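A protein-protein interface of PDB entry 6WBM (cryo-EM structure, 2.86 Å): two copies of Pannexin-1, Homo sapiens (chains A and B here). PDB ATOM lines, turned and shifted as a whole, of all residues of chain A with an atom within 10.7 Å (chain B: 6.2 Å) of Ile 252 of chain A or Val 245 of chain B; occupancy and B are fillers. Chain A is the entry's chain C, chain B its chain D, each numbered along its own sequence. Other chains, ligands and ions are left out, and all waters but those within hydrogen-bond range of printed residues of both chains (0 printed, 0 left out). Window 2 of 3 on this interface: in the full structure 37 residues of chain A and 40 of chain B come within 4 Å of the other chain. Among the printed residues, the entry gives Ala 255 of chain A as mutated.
Of the 14 printed residues of chain A, 6 touch a printed residue of chain B. Hydrophobic or aromatic side chains of chain B within 4 Å of the printed part of chain A: Val 245. Among the printed residues, no Asp or Glu carboxylate lies within 4 Å of a Lys or Arg side-chain nitrogen of the other chain.
Of the printed residues of chain B, Tyr 83 of chain A touches Glu 243 (2.4 Å). Ile 252 of chain A touches just these residues of chain B: Val 245 (3.9 Å), Gln 262 (3.8 Å), Phe 263 (3.6 Å) and Gln 264 (3.0 Å). Ser 93 of chain B touches none of the printed residues of chain A. No residue of chain A comes within 4 Å of Leu 94 of chain B. Gln 95 of chain B touches none of the printed residues of chain A. Of the printed residues of chain A, Glu 243 of chain B touches Tyr 83 (2.4 Å) and Ser 250 (2.7 Å). Val 245 of chain B touches one residue of chain A. No residue of chain A comes within 4 Å of Cys 246 of chain B. Ser 247 of chain B touches none of the printed residues of chain A. Gln 262 of chain B touches one residue of chain A. Gln 264 of chain B touches five residues of chain A. No residue of chain A comes within 4 Å of Cys 265 of chain B. The nearest printed residue of chain B that does not touch Ile 252 of chain A is Cys 246 of chain B (6.1 Å).
Among the printed residues, merely in contact across the chains: Phe 79 of chain A with Gln 264 of chain B (3.8 Å), Ser 250 of chain A with Gln 264 of chain B (3.7 Å), Gly 251 of chain A with Gln 264 of chain B (3.4 Å), Ile 252 of chain A with Val 245 of chain B (3.9 Å), Ile 252 of chain A with Gln 262 of chain B (3.8 Å), Ile 252 of chain A with Phe 263 of chain B (3.6 Å) and Leu 253 of chain A with Gln 264 of chain B (3.8 Å).
O of Cys 246 of chain B is in hydrogen-bond range of N of Phe 263 of chain B, at 2.6 Å. O of Gly 251 of chain A lies within hydrogen-bond range of NH2 of Arg 254 of chain A, at 3.4 Å. N of Gln 95 of chain B is in hydrogen-bond range of O of Val 245 of chain B, at 3.0 Å.
OH of Tyr 83 of chain A lies within hydrogen-bond range of OE2 of Glu 243 of chain B, at 2.4 Å. The backbone NH (N) of Ile 252 of chain A is in hydrogen-bond range of the side-chain amide oxygen (OE1) of Gln 264 of chain B (3.0 Å). The side-chain hydroxyl of Ser 250 of chain A is in hydrogen-bond range of the side-chain carboxylate of Glu 243 of chain B (2.7 Å).
No position is printed for both chains. Of the 10 pairs that touch across the chains among the printed residues, none has its exchanged pair printed and touching as well.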
ATOM      1  N   PHE A  79      25.064   5.179  12.818  1.00  0.00           N
ATOM      2  CA  PHE A  79      24.404   5.964  11.785  1.00  0.00           C
ATOM      3  C   PHE A  79      25.080   7.307  11.604  1.00  0.00           C
ATOM      4  O   PHE A  79      25.265   7.762  10.476  1.00  0.00           O
ATOM      5  CB  PHE A  79      22.932   6.172  12.121  1.00  0.00           C
ATOM      6  CG  PHE A  79      22.276   7.237  11.292  1.00  0.00           C
ATOM      7  CD1 PHE A  79      21.803   6.948  10.031  1.00  0.00           C
ATOM      8  CD2 PHE A  79      22.143   8.524  11.769  1.00  0.00           C
ATOM      9  CE1 PHE A  79      21.206   7.918   9.263  1.00  0.00           C
ATOM     10  CE2 PHE A  79      21.548   9.497  11.002  1.00  0.00           C
ATOM     11  CZ  PHE A  79      21.077   9.193   9.749  1.00  0.00           C
ATOM     12  N   TYR A  83      26.724   8.408   8.162  1.00  0.00           N
ATOM     13  CA  TYR A  83      26.154   9.586   7.530  1.00  0.00           C
ATOM     14  C   TYR A  83      27.230  10.608   7.234  1.00  0.00           C
ATOM     15  O   TYR A  83      27.298  11.140   6.127  1.00  0.00           O
ATOM     16  CB  TYR A  83      25.077  10.202   8.416  1.00  0.00           C
ATOM     17  CG  TYR A  83      24.301  11.311   7.744  1.00  0.00           C
ATOM     18  CD1 TYR A  83      24.889  12.538   7.472  1.00  0.00           C
ATOM     19  CD2 TYR A  83      22.976  11.139   7.397  1.00  0.00           C
ATOM     20  CE1 TYR A  83      24.187  13.546   6.866  1.00  0.00           C
ATOM     21  CE2 TYR A  83      22.265  12.145   6.791  1.00  0.00           C
ATOM     22  CZ  TYR A  83      22.875  13.345   6.528  1.00  0.00           C
ATOM     23  OH  TYR A  83      22.166  14.352   5.923  1.00  0.00           O
ATOM     24  N   ILE A 248      23.660  15.940  11.018  1.00  0.00           N
ATOM     25  CA  ILE A 248      22.575  15.110  10.472  1.00  0.00           C
ATOM     26  C   ILE A 248      21.277  15.856  10.769  1.00  0.00           C
ATOM     27  O   ILE A 248      20.566  15.595  11.740  1.00  0.00           O
ATOM     28  CB  ILE A 248      22.593  13.688  11.040  1.00  0.00           C
ATOM     29  CG1 ILE A 248      22.599  13.700  12.565  1.00  0.00           C
ATOM     30  CG2 ILE A 248      23.834  12.975  10.611  1.00  0.00           C
ATOM     31  CD1 ILE A 248      22.328  12.356  13.175  1.00  0.00           C
ATOM     32  N   LYS A 249      20.948  16.802   9.899  1.00  0.00           N
ATOM     33  CA  LYS A 249      19.725  17.577  10.077  1.00  0.00           C
ATOM     34  C   LYS A 249      19.024  17.773   8.745  1.00  0.00           C
ATOM     35  O   LYS A 249      18.342  18.777   8.522  1.00  0.00           O
ATOM     36  CB  LYS A 249      20.009  18.919  10.745  1.00  0.00           C
ATOM     37  CG  LYS A 249      20.603  18.803  12.136  1.00  0.00           C
ATOM     38  CD  LYS A 249      19.576  18.325  13.143  1.00  0.00           C
ATOM     39  CE  LYS A 249      18.821  19.489  13.747  1.00  0.00           C
ATOM     40  NZ  LYS A 249      18.152  19.105  15.017  1.00  0.00           N
ATOM     41  N   SER A 250      19.183  16.816   7.845  1.00  0.00           N
ATOM     42  CA  SER A 250      18.468  16.810   6.580  1.00  0.00           C
ATOM     43  C   SER A 250      17.284  15.857   6.660  1.00  0.00           C
ATOM     44  O   SER A 250      17.303  14.864   7.389  1.00  0.00           O
ATOM     45  CB  SER A 250      19.398  16.405   5.436  1.00  0.00           C
ATOM     46  OG  SER A 250      19.984  15.141   5.688  1.00  0.00           O
ATOM     47  N   GLY A 251      16.245  16.173   5.897  1.00  0.00           N
ATOM     48  CA  GLY A 251      15.062  15.340   5.942  1.00  0.00           C
ATOM     49  C   GLY A 251      14.268  15.562   7.217  1.00  0.00           C
ATOM     50  O   GLY A 251      14.240  16.657   7.785  1.00  0.00           O
ATOM     51  N   ILE A 252      13.611  14.495   7.674  1.00  0.00           N
ATOM     52  CA  ILE A 252      12.746  14.592   8.844  1.00  0.00           C
ATOM     53  C   ILE A 252      13.503  14.917  10.118  1.00  0.00           C
ATOM     54  O   ILE A 252      12.899  15.417  11.072  1.00  0.00           O
ATOM     55  CB  ILE A 252      11.956  13.285   9.042  1.00  0.00           C
ATOM     56  CG1 ILE A 252      12.914  12.113   9.229  1.00  0.00           C
ATOM     57  CG2 ILE A 252      11.051  13.035   7.859  1.00  0.00           C
ATOM     58  CD1 ILE A 252      12.223  10.794   9.445  1.00  0.00           C
ATOM     59  N   LEU A 253      14.805  14.649  10.165  1.00  0.00           N
ATOM     60  CA  LEU A 253      15.585  14.953  11.354  1.00  0.00           C
ATOM     61  C   LEU A 253      15.733  16.445  11.600  1.00  0.00           C
ATOM     62  O   LEU A 253      16.136  16.836  12.699  1.00  0.00           O
ATOM     63  CB  LEU A 253      16.968  14.316  11.250  1.00  0.00           C
ATOM     64  CG  LEU A 253      16.950  12.793  11.189  1.00  0.00           C
ATOM     65  CD1 LEU A 253      18.358  12.245  11.130  1.00  0.00           C
ATOM     66  CD2 LEU A 253      16.210  12.249  12.387  1.00  0.00           C
ATOM     67  N   ARG A 254      15.419  17.283  10.612  1.00  0.00           N
ATOM     68  CA  ARG A 254      15.556  18.722  10.791  1.00  0.00           C
ATOM     69  C   ARG A 254      14.656  19.226  11.910  1.00  0.00           C
ATOM     70  O   ARG A 254      15.014  20.159  12.636  1.00  0.00           O
ATOM     71  CB  ARG A 254      15.239  19.444   9.485  1.00  0.00           C
ATOM     72  CG  ARG A 254      15.748  20.866   9.429  1.00  0.00           C
ATOM     73  CD  ARG A 254      15.602  21.451   8.036  1.00  0.00           C
ATOM     74  NE  ARG A 254      16.316  20.668   7.031  1.00  0.00           N
ATOM     75  CZ  ARG A 254      15.731  19.820   6.192  1.00  0.00           C
ATOM     76  NH1 ARG A 254      16.460  19.151   5.310  1.00  0.00           N
ATOM     77  NH2 ARG A 254      14.419  19.637   6.239  1.00  0.00           N
ATOM     78  N   ALA A 255      13.481  18.621  12.065  1.00  0.00           N
ATOM     79  CA  ALA A 255      12.579  18.991  13.144  1.00  0.00           C
ATOM     80  C   ALA A 255      12.856  18.229  14.431  1.00  0.00           C
ATOM     81  O   ALA A 255      12.288  18.579  15.471  1.00  0.00           O
ATOM     82  CB  ALA A 255      11.128  18.769  12.716  1.00  0.00           C
ATOM     83  N   ASP A 256      13.697  17.201  14.388  1.00  0.00           N
ATOM     84  CA  ASP A 256      14.002  16.420  15.579  1.00  0.00           C
ATOM     85  C   ASP A 256      14.762  17.280  16.582  1.00  0.00           C
ATOM     86  O   ASP A 256      15.653  18.046  16.204  1.00  0.00           O
ATOM     87  CB  ASP A 256      14.812  15.182  15.209  1.00  0.00           C
ATOM     88  CG  ASP A 256      14.839  14.151  16.318  1.00  0.00           C
ATOM     89  OD1 ASP A 256      15.052  14.533  17.487  1.00  0.00           O
ATOM     90  OD2 ASP A 256      14.641  12.956  16.020  1.00  0.00           O
ATOM     91  N   SER A 257      14.420  17.140  17.866  1.00  0.00           N
ATOM     92  CA  SER A 257      15.045  17.986  18.917  1.00  0.00           C
ATOM     93  C   SER A 257      16.061  17.206  19.762  1.00  0.00           C
ATOM     94  O   SER A 257      16.948  17.857  20.346  1.00  0.00           O
ATOM     95  CB  SER A 257      13.989  18.611  19.788  1.00  0.00           C
ATOM     96  OG  SER A 257      13.194  19.518  19.039  1.00  0.00           O
ATOM     97  N   THR A 258      15.942  15.877  19.831  1.00  0.00           N
ATOM     98  CA  THR A 258      16.861  15.106  20.656  1.00  0.00           C
ATOM     99  C   THR A 258      18.233  14.931  20.022  1.00  0.00           C
ATOM    100  O   THR A 258      19.134  14.392  20.674  1.00  0.00           O
ATOM    101  CB  THR A 258      16.275  13.727  20.957  1.00  0.00           C
ATOM    102  OG1 THR A 258      17.090  13.066  21.933  1.00  0.00           O
ATOM    103  CG2 THR A 258      16.224  12.884  19.695  1.00  0.00           C
ATOM    104  N   VAL A 259      18.414  15.364  18.781  1.00  0.00           N
ATOM    105  CA  VAL A 259      19.693  15.254  18.090  1.00  0.00           C
ATOM    106  C   VAL A 259      20.466  16.548  18.323  1.00  0.00           C
ATOM    107  O   VAL A 259      19.857  17.628  18.300  1.00  0.00           O
ATOM    108  CB  VAL A 259      19.495  14.998  16.594  1.00  0.00           C
ATOM    109  CG1 VAL A 259      19.105  13.565  16.364  1.00  0.00           C
ATOM    110  CG2 VAL A 259      18.417  15.915  16.052  1.00  0.00           C
ATOM    111  N   SER B  93       5.452   1.995   0.780  1.00  0.00           N
ATOM    112  CA  SER B  93       5.898   2.376   2.115  1.00  0.00           C
ATOM    113  C   SER B  93       6.746   3.642   2.095  1.00  0.00           C
ATOM    114  O   SER B  93       6.383   4.644   2.721  1.00  0.00           O
ATOM    115  CB  SER B  93       6.683   1.228   2.749  1.00  0.00           C
ATOM    116  OG  SER B  93       7.867   0.964   2.018  1.00  0.00           O
ATOM    117  N   LEU B  94       7.915   3.559   1.452  1.00  0.00           N
ATOM    118  CA  LEU B  94       8.899   4.679   1.424  1.00  0.00           C
ATOM    119  C   LEU B  94       8.397   5.856   0.578  1.00  0.00           C
ATOM    120  O   LEU B  94       7.677   5.616  -0.410  1.00  0.00           O
ATOM    121  CB  LEU B  94      10.238   4.151   0.901  1.00  0.00           C
ATOM    122  CG  LEU B  94      10.217   3.603  -0.524  1.00  0.00           C
ATOM    123  CD1 LEU B  94      10.278   4.733  -1.538  1.00  0.00           C
ATOM    124  CD2 LEU B  94      11.363   2.628  -0.745  1.00  0.00           C
ATOM    125  N   GLN B  95       8.782   7.075   0.971  1.00  0.00           N
ATOM    126  CA  GLN B  95       8.427   8.305   0.268  1.00  0.00           C
ATOM    127  C   GLN B  95       9.654   9.204   0.233  1.00  0.00           C
ATOM    128  O   GLN B  95      10.074   9.724   1.272  1.00  0.00           O
ATOM    129  CB  GLN B  95       7.252   9.007   0.948  1.00  0.00           C
ATOM    130  N   SER B  96      10.245   9.336  -0.960  1.00  0.00           N
ATOM    131  CA  SER B  96      11.461  10.165  -1.181  1.00  0.00           C
ATOM    132  C   SER B  96      11.126  11.328  -2.124  1.00  0.00           C
ATOM    133  O   SER B  96      10.183  11.182  -2.925  1.00  0.00           O
ATOM    134  CB  SER B  96      12.588   9.324  -1.721  1.00  0.00           C
ATOM    135  OG  SER B  96      13.755  10.107  -1.919  1.00  0.00           O
ATOM    136  N   GLU B 243      19.029   9.895   0.438  1.00  0.00           N
ATOM    137  CA  GLU B 243      18.290  10.070   1.677  1.00  0.00           C
ATOM    138  C   GLU B 243      16.809   9.897   1.381  1.00  0.00           C
ATOM    139  O   GLU B 243      16.247  10.637   0.568  1.00  0.00           O
ATOM    140  CB  GLU B 243      18.550  11.445   2.285  1.00  0.00           C
ATOM    141  CG  GLU B 243      19.930  11.612   2.867  1.00  0.00           C
ATOM    142  CD  GLU B 243      20.104  12.956   3.535  1.00  0.00           C
ATOM    143  OE1 GLU B 243      19.108  13.699   3.632  1.00  0.00           O
ATOM    144  OE2 GLU B 243      21.236  13.272   3.957  1.00  0.00           O
ATOM    145  N   PHE B 244      16.183   8.928   2.036  1.00  0.00           N
ATOM    146  CA  PHE B 244      14.775   8.657   1.817  1.00  0.00           C
ATOM    147  C   PHE B 244      14.113   8.324   3.139  1.00  0.00           C
ATOM    148  O   PHE B 244      14.754   7.828   4.067  1.00  0.00           O
ATOM    149  CB  PHE B 244      14.564   7.508   0.835  1.00  0.00           C
ATOM    150  CG  PHE B 244      15.020   6.183   1.352  1.00  0.00           C
ATOM    151  CD1 PHE B 244      16.359   5.857   1.362  1.00  0.00           C
ATOM    152  CD2 PHE B 244      14.110   5.262   1.823  1.00  0.00           C
ATOM    153  CE1 PHE B 244      16.781   4.640   1.831  1.00  0.00           C
ATOM    154  CE2 PHE B 244      14.527   4.043   2.295  1.00  0.00           C
ATOM    155  CZ  PHE B 244      15.865   3.732   2.298  1.00  0.00           C
ATOM    156  N   VAL B 245      12.818   8.594   3.210  1.00  0.00           N
ATOM    157  CA  VAL B 245      12.029   8.370   4.410  1.00  0.00           C
ATOM    158  C   VAL B 245      11.350   7.017   4.300  1.00  0.00           C
ATOM    159  O   VAL B 245      10.594   6.768   3.356  1.00  0.00           O
ATOM    160  CB  VAL B 245      10.996   9.489   4.603  1.00  0.00           C
ATOM    161  CG1 VAL B 245      10.153   9.205   5.810  1.00  0.00           C
ATOM    162  CG2 VAL B 245      11.700  10.819   4.749  1.00  0.00           C
ATOM    163  N   CYS B 246      11.606   6.148   5.271  1.00  0.00           N
ATOM    164  CA  CYS B 246      11.069   4.799   5.280  1.00  0.00           C
ATOM    165  C   CYS B 246      10.188   4.622   6.506  1.00  0.00           C
ATOM    166  O   CYS B 246      10.396   5.270   7.533  1.00  0.00           O
ATOM    167  CB  CYS B 246      12.194   3.765   5.269  1.00  0.00           C
ATOM    168  SG  CYS B 246      11.787   2.173   5.976  1.00  0.00           S
ATOM    169  N   SER B 247       9.197   3.741   6.392  1.00  0.00           N
ATOM    170  CA  SER B 247       8.184   3.578   7.427  1.00  0.00           C
ATOM    171  C   SER B 247       7.855   2.104   7.595  1.00  0.00           C
ATOM    172  O   SER B 247       7.337   1.474   6.669  1.00  0.00           O
ATOM    173  CB  SER B 247       6.922   4.364   7.079  1.00  0.00           C
ATOM    174  OG  SER B 247       5.823   3.922   7.852  1.00  0.00           O
ATOM    175  N   GLN B 262       7.955   7.267  10.910  1.00  0.00           N
ATOM    176  CA  GLN B 262       8.865   7.138   9.785  1.00  0.00           C
ATOM    177  C   GLN B 262      10.296   7.314  10.262  1.00  0.00           C
ATOM    178  O   GLN B 262      10.551   7.957  11.281  1.00  0.00           O
ATOM    179  CB  GLN B 262       8.540   8.160   8.701  1.00  0.00           C
ATOM    180  CG  GLN B 262       8.190   9.520   9.247  1.00  0.00           C
ATOM    181  CD  GLN B 262       7.475  10.381   8.233  1.00  0.00           C
ATOM    182  OE1 GLN B 262       7.235   9.959   7.104  1.00  0.00           O
ATOM    183  NE2 GLN B 262       7.129  11.597   8.632  1.00  0.00           N
ATOM    184  N   PHE B 263      11.221   6.738   9.505  1.00  0.00           N
ATOM    185  CA  PHE B 263      12.637   6.768   9.824  1.00  0.00           C
ATOM    186  C   PHE B 263      13.397   7.455   8.702  1.00  0.00           C
ATOM    187  O   PHE B 263      13.026   7.353   7.531  1.00  0.00           O
ATOM    188  CB  PHE B 263      13.196   5.360  10.026  1.00  0.00           C
ATOM    189  CG  PHE B 263      12.519   4.587  11.115  1.00  0.00           C
ATOM    190  CD1 PHE B 263      11.270   4.041  10.921  1.00  0.00           C
ATOM    191  CD2 PHE B 263      13.139   4.397  12.332  1.00  0.00           C
ATOM    192  CE1 PHE B 263      10.648   3.332  11.917  1.00  0.00           C
ATOM    193  CE2 PHE B 263      12.519   3.684  13.332  1.00  0.00           C
ATOM    194  CZ  PHE B 263      11.275   3.150  13.122  1.00  0.00           C
ATOM    195  N   GLN B 264      14.467   8.148   9.068  1.00  0.00           N
ATOM    196  CA  GLN B 264      15.311   8.857   8.112  1.00  0.00           C
ATOM    197  C   GLN B 264      16.486   7.958   7.755  1.00  0.00           C
ATOM    198  O   GLN B 264      17.463   7.874   8.499  1.00  0.00           O
ATOM    199  CB  GLN B 264      15.795  10.180   8.685  1.00  0.00           C
ATOM    200  CG  GLN B 264      16.790  10.888   7.796  1.00  0.00           C
ATOM    201  CD  GLN B 264      16.144  11.436   6.551  1.00  0.00           C
ATOM    202  OE1 GLN B 264      15.079  12.043   6.612  1.00  0.00           O
ATOM    203  NE2 GLN B 264      16.784  11.226   5.410  1.00  0.00           N
ATOM    204  N   CYS B 265      16.395   7.294   6.615  1.00  0.00           N
ATOM    205  CA  CYS B 265      17.453   6.415   6.153  1.00  0.00           C
ATOM    206  C   CYS B 265      18.335   7.152   5.159  1.00  0.00           C
ATOM    207  O   CYS B 265      17.924   8.146   4.561  1.00  0.00           O
ATOM    208  CB  CYS B 265      16.871   5.162   5.506  1.00  0.00           C
ATOM    209  SG  CYS B 265      15.781   4.246   6.598  1.00  0.00           S
